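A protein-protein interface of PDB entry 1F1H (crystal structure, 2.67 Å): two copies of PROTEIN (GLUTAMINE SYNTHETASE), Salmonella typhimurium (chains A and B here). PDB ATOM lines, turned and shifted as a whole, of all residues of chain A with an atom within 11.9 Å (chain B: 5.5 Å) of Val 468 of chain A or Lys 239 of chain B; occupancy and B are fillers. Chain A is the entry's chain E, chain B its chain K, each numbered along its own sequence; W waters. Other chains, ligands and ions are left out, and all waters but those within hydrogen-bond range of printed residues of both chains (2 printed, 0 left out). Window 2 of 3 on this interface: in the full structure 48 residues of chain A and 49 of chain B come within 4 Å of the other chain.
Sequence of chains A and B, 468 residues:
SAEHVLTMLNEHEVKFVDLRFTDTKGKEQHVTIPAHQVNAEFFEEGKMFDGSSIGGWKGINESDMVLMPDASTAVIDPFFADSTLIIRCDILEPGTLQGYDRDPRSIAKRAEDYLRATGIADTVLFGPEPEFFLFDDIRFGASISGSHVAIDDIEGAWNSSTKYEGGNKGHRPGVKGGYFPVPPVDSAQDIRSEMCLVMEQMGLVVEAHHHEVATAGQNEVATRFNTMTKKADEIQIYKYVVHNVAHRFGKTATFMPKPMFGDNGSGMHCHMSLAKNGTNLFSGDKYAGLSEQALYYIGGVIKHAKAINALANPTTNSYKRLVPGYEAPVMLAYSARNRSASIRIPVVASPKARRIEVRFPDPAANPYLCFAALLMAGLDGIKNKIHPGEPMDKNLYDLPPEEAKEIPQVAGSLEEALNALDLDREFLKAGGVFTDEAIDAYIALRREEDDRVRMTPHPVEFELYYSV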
ATOM      1  N   VAL A 460      -9.600   0.881  32.136  1.00  0.00           N
ATOM      2  CA  VAL A 460      -9.857   1.240  30.739  1.00  0.00           C
ATOM      3  C   VAL A 460      -9.963   2.760  30.514  1.00  0.00           C
ATOM      4  O   VAL A 460      -9.689   3.273  29.417  1.00  0.00           O
ATOM      5  CB  VAL A 460     -11.122   0.484  30.221  1.00  0.00           C
ATOM      6  CG1 VAL A 460     -11.582   1.010  28.885  1.00  0.00           C
ATOM      7  CG2 VAL A 460     -10.801  -1.000  30.070  1.00  0.00           C
ATOM      8  N   GLU A 461     -10.318   3.481  31.572  1.00  0.00           N
ATOM      9  CA  GLU A 461     -10.437   4.937  31.503  1.00  0.00           C
ATOM     10  C   GLU A 461      -9.069   5.578  31.327  1.00  0.00           C
ATOM     11  O   GLU A 461      -8.944   6.686  30.818  1.00  0.00           O
ATOM     12  CB  GLU A 461     -11.135   5.483  32.753  1.00  0.00           C
ATOM     13  CG  GLU A 461     -12.618   5.087  32.831  1.00  0.00           C
ATOM     14  CD  GLU A 461     -13.373   5.690  34.018  1.00  0.00           C
ATOM     15  OE1 GLU A 461     -14.580   5.963  33.868  1.00  0.00           O
ATOM     16  OE2 GLU A 461     -12.789   5.864  35.108  1.00  0.00           O
ATOM     17  N   PHE A 462      -8.038   4.860  31.758  1.00  0.00           N
ATOM     18  CA  PHE A 462      -6.684   5.343  31.596  1.00  0.00           C
ATOM     19  C   PHE A 462      -6.215   5.116  30.176  1.00  0.00           C
ATOM     20  O   PHE A 462      -5.529   5.958  29.588  1.00  0.00           O
ATOM     21  CB  PHE A 462      -5.748   4.652  32.607  1.00  0.00           C
ATOM     22  CG  PHE A 462      -6.071   5.112  34.004  1.00  0.00           C
ATOM     23  CD1 PHE A 462      -5.326   6.152  34.567  1.00  0.00           C
ATOM     24  CD2 PHE A 462      -7.108   4.557  34.741  1.00  0.00           C
ATOM     25  CE1 PHE A 462      -5.632   6.631  35.836  1.00  0.00           C
ATOM     26  CE2 PHE A 462      -7.411   5.040  36.020  1.00  0.00           C
ATOM     27  CZ  PHE A 462      -6.685   6.070  36.561  1.00  0.00           C
ATOM     28  N   GLU A 463      -6.604   3.970  29.625  1.00  0.00           N
ATOM     29  CA  GLU A 463      -6.255   3.570  28.264  1.00  0.00           C
ATOM     30  C   GLU A 463      -6.829   4.618  27.327  1.00  0.00           C
ATOM     31  O   GLU A 463      -6.153   5.116  26.421  1.00  0.00           O
ATOM     32  CB  GLU A 463      -6.901   2.211  27.971  1.00  0.00           C
ATOM     33  CG  GLU A 463      -6.410   1.470  26.739  1.00  0.00           C
ATOM     34  CD  GLU A 463      -6.523  -0.014  26.930  1.00  0.00           C
ATOM     35  OE1 GLU A 463      -5.516  -0.668  27.296  1.00  0.00           O
ATOM     36  OE2 GLU A 463      -7.639  -0.523  26.731  1.00  0.00           O
ATOM     37  N   LEU A 464      -8.073   4.976  27.626  1.00  0.00           N
ATOM     38  CA  LEU A 464      -8.897   5.949  26.877  1.00  0.00           C
ATOM     39  C   LEU A 464      -8.605   7.414  27.171  1.00  0.00           C
ATOM     40  O   LEU A 464      -8.637   8.234  26.261  1.00  0.00           O
ATOM     41  CB  LEU A 464     -10.377   5.735  27.238  1.00  0.00           C
ATOM     42  CG  LEU A 464     -11.349   4.979  26.316  1.00  0.00           C
ATOM     43  CD1 LEU A 464     -10.608   4.024  25.405  1.00  0.00           C
ATOM     44  CD2 LEU A 464     -12.395   4.240  27.138  1.00  0.00           C
ATOM     45  N   TYR A 465      -8.329   7.791  28.421  1.00  0.00           N
ATOM     46  CA  TYR A 465      -8.217   9.214  28.761  1.00  0.00           C
ATOM     47  C   TYR A 465      -6.946   9.743  29.402  1.00  0.00           C
ATOM     48  O   TYR A 465      -6.847  10.964  29.603  1.00  0.00           O
ATOM     49  CB  TYR A 465      -9.378   9.566  29.666  1.00  0.00           C
ATOM     50  CG  TYR A 465     -10.723   9.091  29.171  1.00  0.00           C
ATOM     51  CD1 TYR A 465     -11.218   9.491  27.924  1.00  0.00           C
ATOM     52  CD2 TYR A 465     -11.511   8.249  29.955  1.00  0.00           C
ATOM     53  CE1 TYR A 465     -12.470   9.066  27.476  1.00  0.00           C
ATOM     54  CE2 TYR A 465     -12.762   7.818  29.516  1.00  0.00           C
ATOM     55  CZ  TYR A 465     -13.235   8.234  28.284  1.00  0.00           C
ATOM     56  OH  TYR A 465     -14.480   7.811  27.855  1.00  0.00           O
ATOM     57  N   TYR A 466      -5.983   8.908  29.725  1.00  0.00           N
ATOM     58  CA  TYR A 466      -4.810   9.472  30.389  1.00  0.00           C
ATOM     59  C   TYR A 466      -4.107  10.591  29.599  1.00  0.00           C
ATOM     60  O   TYR A 466      -3.652  11.564  30.190  1.00  0.00           O
ATOM     61  CB  TYR A 466      -3.836   8.356  30.762  1.00  0.00           C
ATOM     62  CG  TYR A 466      -2.646   8.836  31.571  1.00  0.00           C
ATOM     63  CD1 TYR A 466      -2.744   9.022  32.949  1.00  0.00           C
ATOM     64  CD2 TYR A 466      -1.422   9.104  30.957  1.00  0.00           C
ATOM     65  CE1 TYR A 466      -1.654   9.456  33.699  1.00  0.00           C
ATOM     66  CE2 TYR A 466      -0.323   9.542  31.697  1.00  0.00           C
ATOM     67  CZ  TYR A 466      -0.444   9.713  33.065  1.00  0.00           C
ATOM     68  OH  TYR A 466       0.644  10.135  33.793  1.00  0.00           O
ATOM     69  N   SER A 467      -4.028  10.460  28.275  1.00  0.00           N
ATOM     70  CA  SER A 467      -3.346  11.450  27.440  1.00  0.00           C
ATOM     71  C   SER A 467      -4.255  12.553  26.932  1.00  0.00           C
ATOM     72  O   SER A 467      -3.926  13.268  25.985  1.00  0.00           O
ATOM     73  CB  SER A 467      -2.686  10.760  26.248  1.00  0.00           C
ATOM     74  OG  SER A 467      -1.653   9.898  26.659  1.00  0.00           O
ATOM     75  N   VAL A 468      -5.373  12.727  27.605  1.00  0.00           N
ATOM     76  CA  VAL A 468      -6.361  13.723  27.230  1.00  0.00           C
ATOM     77  C   VAL A 468      -5.848  15.173  27.282  1.00  0.00           C
ATOM     78  O   VAL A 468      -4.935  15.475  28.085  1.00  0.00           O
ATOM     79  CB  VAL A 468      -7.633  13.493  28.090  1.00  0.00           C
ATOM     80  CG1 VAL A 468      -7.775  14.530  29.166  1.00  0.00           C
ATOM     81  CG2 VAL A 468      -8.842  13.361  27.219  1.00  0.00           C
ATOM     82  OXT VAL A 468      -6.341  15.989  26.474  1.00  0.00           O
ATOM     83  N   GLY B  26     -10.548  16.568  20.853  1.00  0.00           N
ATOM     84  CA  GLY B  26      -9.867  17.683  21.499  1.00  0.00           C
ATOM     85  C   GLY B  26      -8.361  17.597  21.634  1.00  0.00           C
ATOM     86  O   GLY B  26      -7.737  18.426  22.319  1.00  0.00           O
ATOM     87  N   LYS B  27      -7.785  16.597  20.969  1.00  0.00           N
ATOM     88  CA  LYS B  27      -6.355  16.359  21.015  1.00  0.00           C
ATOM     89  C   LYS B  27      -5.642  17.106  19.899  1.00  0.00           C
ATOM     90  O   LYS B  27      -5.996  16.980  18.731  1.00  0.00           O
ATOM     91  CB  LYS B  27      -6.071  14.852  20.913  1.00  0.00           C
ATOM     92  CG  LYS B  27      -4.622  14.455  21.199  1.00  0.00           C
ATOM     93  CD  LYS B  27      -4.292  14.561  22.683  1.00  0.00           C
ATOM     94  CE  LYS B  27      -2.796  14.676  22.911  1.00  0.00           C
ATOM     95  NZ  LYS B  27      -2.432  14.932  24.339  1.00  0.00           N
ATOM     96  N   GLU B 234      -5.167  28.767  23.535  1.00  0.00           N
ATOM     97  CA  GLU B 234      -4.308  28.844  24.707  1.00  0.00           C
ATOM     98  C   GLU B 234      -4.387  27.579  25.554  1.00  0.00           C
ATOM     99  O   GLU B 234      -3.364  27.136  26.073  1.00  0.00           O
ATOM    100  CB  GLU B 234      -4.627  30.099  25.533  1.00  0.00           C
ATOM    101  CG  GLU B 234      -4.359  31.408  24.757  1.00  0.00           C
ATOM    102  CD  GLU B 234      -4.331  32.663  25.624  1.00  0.00           C
ATOM    103  OE1 GLU B 234      -4.757  32.598  26.796  1.00  0.00           O
ATOM    104  OE2 GLU B 234      -3.867  33.718  25.133  1.00  0.00           O
ATOM    105  N   ILE B 235      -5.579  26.980  25.656  1.00  0.00           N
ATOM    106  CA  ILE B 235      -5.749  25.748  26.421  1.00  0.00           C
ATOM    107  C   ILE B 235      -4.921  24.635  25.784  1.00  0.00           C
ATOM    108  O   ILE B 235      -4.278  23.844  26.481  1.00  0.00           O
ATOM    109  CB  ILE B 235      -7.230  25.312  26.515  1.00  0.00           C
ATOM    110  CG1 ILE B 235      -7.952  26.130  27.591  1.00  0.00           C
ATOM    111  CG2 ILE B 235      -7.349  23.816  26.813  1.00  0.00           C
ATOM    112  CD1 ILE B 235      -7.464  25.902  29.004  1.00  0.00           C
ATOM    113  N   GLN B 236      -4.934  24.572  24.461  1.00  0.00           N
ATOM    114  CA  GLN B 236      -4.147  23.567  23.770  1.00  0.00           C
ATOM    115  C   GLN B 236      -2.649  23.803  24.003  1.00  0.00           C
ATOM    116  O   GLN B 236      -1.903  22.849  24.216  1.00  0.00           O
ATOM    117  CB  GLN B 236      -4.482  23.558  22.284  1.00  0.00           C
ATOM    118  CG  GLN B 236      -5.916  23.168  22.018  1.00  0.00           C
ATOM    119  CD  GLN B 236      -6.215  21.724  22.355  1.00  0.00           C
ATOM    120  OE1 GLN B 236      -6.523  21.376  23.507  1.00  0.00           O
ATOM    121  NE2 GLN B 236      -6.165  20.872  21.339  1.00  0.00           N
ATOM    122  N   ILE B 237      -2.223  25.066  23.992  1.00  0.00           N
ATOM    123  CA  ILE B 237      -0.818  25.430  24.234  1.00  0.00           C
ATOM    124  C   ILE B 237      -0.484  25.113  25.695  1.00  0.00           C
ATOM    125  O   ILE B 237       0.589  24.595  25.997  1.00  0.00           O
ATOM    126  CB  ILE B 237      -0.572  26.946  23.949  1.00  0.00           C
ATOM    127  CG1 ILE B 237      -0.622  27.216  22.443  1.00  0.00           C
ATOM    128  CG2 ILE B 237       0.768  27.412  24.515  1.00  0.00           C
ATOM    129  CD1 ILE B 237      -0.670  28.677  22.090  1.00  0.00           C
ATOM    130  N   TYR B 238      -1.424  25.412  26.590  1.00  0.00           N
ATOM    131  CA  TYR B 238      -1.292  25.141  28.023  1.00  0.00           C
ATOM    132  C   TYR B 238      -1.038  23.641  28.220  1.00  0.00           C
ATOM    133  O   TYR B 238      -0.038  23.249  28.821  1.00  0.00           O
ATOM    134  CB  TYR B 238      -2.591  25.555  28.730  1.00  0.00           C
ATOM    135  CG  TYR B 238      -2.650  25.352  30.231  1.00  0.00           C
ATOM    136  CD1 TYR B 238      -2.910  24.093  30.780  1.00  0.00           C
ATOM    137  CD2 TYR B 238      -2.527  26.437  31.105  1.00  0.00           C
ATOM    138  CE1 TYR B 238      -3.047  23.916  32.164  1.00  0.00           C
ATOM    139  CE2 TYR B 238      -2.661  26.274  32.488  1.00  0.00           C
ATOM    140  CZ  TYR B 238      -2.925  25.009  33.009  1.00  0.00           C
ATOM    141  OH  TYR B 238      -3.070  24.839  34.368  1.00  0.00           O
ATOM    142  N   LYS B 239      -1.937  22.802  27.710  1.00  0.00           N
ATOM    143  CA  LYS B 239      -1.771  21.360  27.839  1.00  0.00           C
ATOM    144  C   LYS B 239      -0.419  20.910  27.254  1.00  0.00           C
ATOM    145  O   LYS B 239       0.258  20.057  27.830  1.00  0.00           O
ATOM    146  CB  LYS B 239      -2.910  20.601  27.142  1.00  0.00           C
ATOM    147  CG  LYS B 239      -4.302  20.576  27.827  1.00  0.00           C
ATOM    148  CD  LYS B 239      -5.228  19.708  26.970  1.00  0.00           C
ATOM    149  CE  LYS B 239      -6.639  19.525  27.496  1.00  0.00           C
ATOM    150  NZ  LYS B 239      -7.459  19.039  26.330  1.00  0.00           N
ATOM    151  N   TYR B 240      -0.017  21.501  26.129  1.00  0.00           N
ATOM    152  CA  TYR B 240       1.248  21.136  25.481  1.00  0.00           C
ATOM    153  C   TYR B 240       2.436  21.419  26.395  1.00  0.00           C
ATOM    154  O   TYR B 240       3.294  20.552  26.594  1.00  0.00           O
ATOM    155  CB  TYR B 240       1.410  21.875  24.146  1.00  0.00           C
ATOM    156  CG  TYR B 240       2.665  21.524  23.363  1.00  0.00           C
ATOM    157  CD1 TYR B 240       2.812  20.270  22.765  1.00  0.00           C
ATOM    158  CD2 TYR B 240       3.717  22.443  23.237  1.00  0.00           C
ATOM    159  CE1 TYR B 240       3.981  19.931  22.061  1.00  0.00           C
ATOM    160  CE2 TYR B 240       4.889  22.115  22.537  1.00  0.00           C
ATOM    161  CZ  TYR B 240       5.015  20.858  21.955  1.00  0.00           C
ATOM    162  OH  TYR B 240       6.188  20.509  21.314  1.00  0.00           O
ATOM    163  N   VAL B 241       2.489  22.629  26.942  1.00  0.00           N
ATOM    164  CA  VAL B 241       3.567  23.003  27.849  1.00  0.00           C
ATOM    165  C   VAL B 241       3.572  22.115  29.091  1.00  0.00           C
ATOM    166  O   VAL B 241       4.624  21.622  29.491  1.00  0.00           O
ATOM    167  CB  VAL B 241       3.469  24.482  28.263  1.00  0.00           C
ATOM    168  CG1 VAL B 241       4.488  24.803  29.349  1.00  0.00           C
ATOM    169  CG2 VAL B 241       3.717  25.358  27.058  1.00  0.00           C
ATOM    170  N   VAL B 242       2.404  21.888  29.686  1.00  0.00           N
ATOM    171  CA  VAL B 242       2.319  21.043  30.878  1.00  0.00           C
ATOM    172  C   VAL B 242       2.840  19.637  30.586  1.00  0.00           C
ATOM    173  O   VAL B 242       3.754  19.153  31.258  1.00  0.00           O
ATOM    174  CB  VAL B 242       0.880  20.958  31.418  1.00  0.00           C
ATOM    175  CG1 VAL B 242       0.796  19.904  32.503  1.00  0.00           C
ATOM    176  CG2 VAL B 242       0.452  22.312  31.977  1.00  0.00           C
ATOM    177  N   HIS B 243       2.289  19.009  29.551  1.00  0.00           N
ATOM    178  CA  HIS B 243       2.703  17.666  29.152  1.00  0.00           C
ATOM    179  C   HIS B 243       4.211  17.575  28.900  1.00  0.00           C
ATOM    180  O   HIS B 243       4.897  16.727  29.470  1.00  0.00           O
ATOM    181  CB  HIS B 243       1.939  17.235  27.901  1.00  0.00           C
ATOM    182  CG  HIS B 243       0.576  16.684  28.179  1.00  0.00           C
ATOM    183  ND1 HIS B 243      -0.517  16.962  27.381  1.00  0.00           N
ATOM    184  CD2 HIS B 243       0.133  15.825  29.127  1.00  0.00           C
ATOM    185  CE1 HIS B 243      -1.567  16.294  27.825  1.00  0.00           C
ATOM    186  NE2 HIS B 243      -1.197  15.597  28.884  1.00  0.00           N
ATOM    187  N   ASN B 244       4.740  18.504  28.114  1.00  0.00           N
ATOM    188  CA  ASN B 244       6.159  18.495  27.789  1.00  0.00           C
ATOM    189  C   ASN B 244       7.169  18.960  28.833  1.00  0.00           C
ATOM    190  O   ASN B 244       8.315  18.503  28.829  1.00  0.00           O
ATOM    191  CB  ASN B 244       6.389  19.177  26.458  1.00  0.00           C
ATOM    192  CG  ASN B 244       5.940  18.319  25.307  1.00  0.00           C
ATOM    193  OD1 ASN B 244       4.795  18.416  24.851  1.00  0.00           O
ATOM    194  ND2 ASN B 244       6.823  17.421  24.863  1.00  0.00           N
ATOM    195  N   THR B 254      -1.238  14.366  33.493  1.00  0.00           N
ATOM    196  CA  THR B 254      -2.532  13.954  32.964  1.00  0.00           C
ATOM    197  C   THR B 254      -3.602  14.967  33.296  1.00  0.00           C
ATOM    198  O   THR B 254      -3.566  15.622  34.342  1.00  0.00           O
ATOM    199  CB  THR B 254      -2.988  12.556  33.457  1.00  0.00           C
ATOM    200  OG1 THR B 254      -4.244  12.223  32.849  1.00  0.00           O
ATOM    201  CG2 THR B 254      -3.167  12.543  34.950  1.00  0.00           C
ATOM    202  N   PHE B 255      -4.515  15.136  32.353  1.00  0.00           N
ATOM    203  CA  PHE B 255      -5.627  16.031  32.533  1.00  0.00           C
ATOM    204  C   PHE B 255      -6.912  15.255  32.784  1.00  0.00           C
ATOM    205  O   PHE B 255      -7.989  15.824  32.715  1.00  0.00           O
ATOM    206  CB  PHE B 255      -5.749  16.959  31.339  1.00  0.00           C
ATOM    207  CG  PHE B 255      -4.717  18.038  31.330  1.00  0.00           C
ATOM    208  CD1 PHE B 255      -4.906  19.193  32.080  1.00  0.00           C
ATOM    209  CD2 PHE B 255      -3.544  17.891  30.602  1.00  0.00           C
ATOM    210  CE1 PHE B 255      -3.936  20.194  32.104  1.00  0.00           C
ATOM    211  CE2 PHE B 255      -2.566  18.887  30.618  1.00  0.00           C
ATOM    212  CZ  PHE B 255      -2.762  20.038  31.371  1.00  0.00           C
ATOM    213  N   MET B 256      -6.794  13.954  33.059  1.00  0.00           N
ATOM    214  CA  MET B 256      -7.954  13.115  33.370  1.00  0.00           C
ATOM    215  C   MET B 256      -8.695  13.771  34.519  1.00  0.00           C
ATOM    216  O   MET B 256      -8.085  14.214  35.503  1.00  0.00           O
ATOM    217  CB  MET B 256      -7.546  11.765  33.936  1.00  0.00           C
ATOM    218  CG  MET B 256      -7.017  10.754  33.009  1.00  0.00           C
ATOM    219  SD  MET B 256      -6.654   9.380  34.082  1.00  0.00           S
ATOM    220  CE  MET B 256      -8.238   8.559  34.067  1.00  0.00           C
ATOM    221  N   PRO B 257     -10.023  13.718  34.479  1.00  0.00           N
ATOM    222  CA  PRO B 257     -10.848  14.312  35.528  1.00  0.00           C
ATOM    223  C   PRO B 257     -10.713  13.637  36.904  1.00  0.00           C
ATOM    224  O   PRO B 257     -10.648  14.323  37.929  1.00  0.00           O
ATOM    225  CB  PRO B 257     -12.267  14.153  34.973  1.00  0.00           C
ATOM    226  CG  PRO B 257     -12.062  14.037  33.488  1.00  0.00           C
ATOM    227  CD  PRO B 257     -10.851  13.188  33.386  1.00  0.00           C
ATOM    228  N   THR B 315     -15.942  12.393  29.019  1.00  0.00           N
ATOM    229  CA  THR B 315     -15.409  11.065  29.329  1.00  0.00           C
ATOM    230  C   THR B 315     -16.230  10.378  30.403  1.00  0.00           C
ATOM    231  O   THR B 315     -16.877  11.047  31.209  1.00  0.00           O
ATOM    232  CB  THR B 315     -13.955  11.170  29.858  1.00  0.00           C
ATOM    233  OG1 THR B 315     -13.958  11.678  31.201  1.00  0.00           O
ATOM    234  CG2 THR B 315     -13.147  12.116  29.002  1.00  0.00           C
ATOM    235  N   PRO B 363     -10.919  19.253  32.413  1.00  0.00           N
ATOM    236  CA  PRO B 363      -9.907  19.392  31.363  1.00  0.00           C
ATOM    237  C   PRO B 363      -9.943  18.437  30.159  1.00  0.00           C
ATOM    238  O   PRO B 363      -9.222  18.659  29.174  1.00  0.00           O
ATOM    239  CB  PRO B 363      -8.594  19.254  32.144  1.00  0.00           C
ATOM    240  CG  PRO B 363      -8.967  19.632  33.547  1.00  0.00           C
ATOM    241  CD  PRO B 363     -10.285  18.959  33.708  1.00  0.00           C
ATOM    242  N   ALA B 364     -10.739  17.370  30.233  1.00  0.00           N
ATOM    243  CA  ALA B 364     -10.819  16.401  29.130  1.00  0.00           C
ATOM    244  C   ALA B 364     -11.650  16.943  27.983  1.00  0.00           C
ATOM    245  O   ALA B 364     -11.659  16.404  26.873  1.00  0.00           O
ATOM    246  CB  ALA B 364     -11.405  15.089  29.620  1.00  0.00           C
ATOM    247  N   ALA B 365     -12.372  18.005  28.290  1.00  0.00           N
ATOM    248  CA  ALA B 365     -13.239  18.668  27.350  1.00  0.00           C
ATOM    249  C   ALA B 365     -12.469  19.311  26.216  1.00  0.00           C
ATOM    250  O   ALA B 365     -11.401  19.886  26.421  1.00  0.00           O
ATOM    251  CB  ALA B 365     -14.027  19.735  28.077  1.00  0.00           C
ATOM    252  N   PRO B 367     -11.686  22.128  24.385  1.00  0.00           N
ATOM    253  CA  PRO B 367     -11.940  23.544  24.683  1.00  0.00           C
ATOM    254  C   PRO B 367     -12.842  24.272  23.682  1.00  0.00           C
ATOM    255  O   PRO B 367     -13.749  24.995  24.080  1.00  0.00           O
ATOM    256  CB  PRO B 367     -10.533  24.139  24.775  1.00  0.00           C
ATOM    257  CG  PRO B 367      -9.734  23.273  23.849  1.00  0.00           C
ATOM    258  CD  PRO B 367     -10.249  21.887  24.185  1.00  0.00           C
HETATM  259  O   HOH W   1      -3.274  14.258  29.915  1.00  0.00           O
HETATM  260  O   HOH W   2      -3.913  16.994  25.401  1.00  0.00           O
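The backbone carbonyl oxygen (O) of Ser 467 of chain A lies within hydrogen-bond range of the side-chain amino group (NZ) of Lys 27 of chain B, 2.8 Å away.
The chain-end carboxylate (OXT) of Val 468 of chain A lies within salt-bridge range of the side-chain amino group (NZ) of Lys 239 of chain B, 3.3 Å away.
The backbone carbonyl oxygen (O) of Tyr 466 of chain A lies within hydrogen-bond range of the side-chain hydroxyl (OG1) of Thr 254 of chain B (2.8 Å).
The backbone carbonyl oxygen (O) of Lys 239 of chain B is in hydrogen-bond range of a ring nitrogen (ND1) of His 243 of chain B.
The side-chain hydroxyl of Thr 254 of chain B sits at hydrogen-bond distance from the backbone NH of Met 256 of chain B, at 3.1 Å.
NZ of Lys 239 of chain B lies close to O of Pro 363 of chain B (3.4 Å).
Among the printed residues, merely in contact across the chains: Tyr 465 of chain A with Thr 315 of chain B (3.4 Å), Tyr 465 of chain A with Met 256 of chain B (3.4 Å), Phe 462 of chain A with Met 256 of chain B (3.4 Å), Val 468 of chain A with His 243 of chain B (3.5 Å), Val 468 of chain A with Ala 364 of chain B (3.6 Å), Tyr 466 of chain A with Met 256 of chain B (3.7 Å), Val 468 of chain A with Phe 255 of chain B (3.7 Å) and Glu 461 of chain A with Met 256 of chain B (3.8 Å).
Of the printed residues of chain B, Phe 462 of chain A touches Met 256.
Printed residues of chain B within 4 Å of Ser 467 of chain A: Lys 27.
Val 468 of chain A touches just these residues of chain B: Lys 239, His 243, Phe 255 and Ala 364.
No residue of chain A comes within 4 Å of Gly 26 of chain B.
Of the printed residues of chain A, Lys 27 of chain B touches Ser 467.
No residue of chain A comes within 4 Å of Ile 235 of chain B.
No residue of chain A comes within 4 Å of Tyr 238 of chain B.
Of the printed residues of chain A, Lys 239 of chain B touches Val 468 (3.3 Å).
No residue of chain A comes within 4 Å of Val 241 of chain B.
No residue of chain A comes within 4 Å of Val 242 of chain B.
Of the printed residues of chain A, Phe 255 of chain B touches Val 468 (3.7 Å).
Met 256 of chain B touches four residues of chain A.
No residue of chain A comes within 4 Å of Pro 363 of chain B.
Ala 365 of chain B touches none of the printed residues of chain A.
The nearest residue of chain B that does not touch Val 468 of chain A is Met 256 of chain B (4.1 Å).
The nearest residue of chain A that does not touch Lys 239 of chain B is Ser 467 of chain A (6.6 Å).
Of the 22 printed residues of chain B, 8 touch a printed residue of chain A.
Printed residues of chain B that touch a printed residue of chain A: Lys 27, Lys 239, His 243, Thr 254, Phe 255, Met 256, Thr 315 and Ala 364.
Hydrophobic or aromatic side chains of chain B that line the printed part of chain A: His 243, Phe 255, Met 256 and Ala 364.
Among the printed residues, no Asp or Glu carboxylate lies within 4 Å of a Lys or Arg side-chain nitrogen of the other chain.
No position is printed for both chains.
Of the 11 pairs that touch across the chains among the printed residues, none has its exchanged pair printed and touching as well.
Water W1 lies within hydrogen-bond range of a ring nitrogen (NE2) of His 243 of chain B (2.7 Å), the backbone carbonyl oxygen (O) of Tyr 466 of chain A (2.7 Å), the chain-end carboxylate (O) of Val 468 of chain A (2.8 Å) and the backbone NH (N) of Phe 255 of chain B (2.9 Å).
Water W2 lies within hydrogen-bond range of NZ of Lys 27 of chain B (2.8 Å) and OXT of Val 468 of chain A (2.8 Å).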
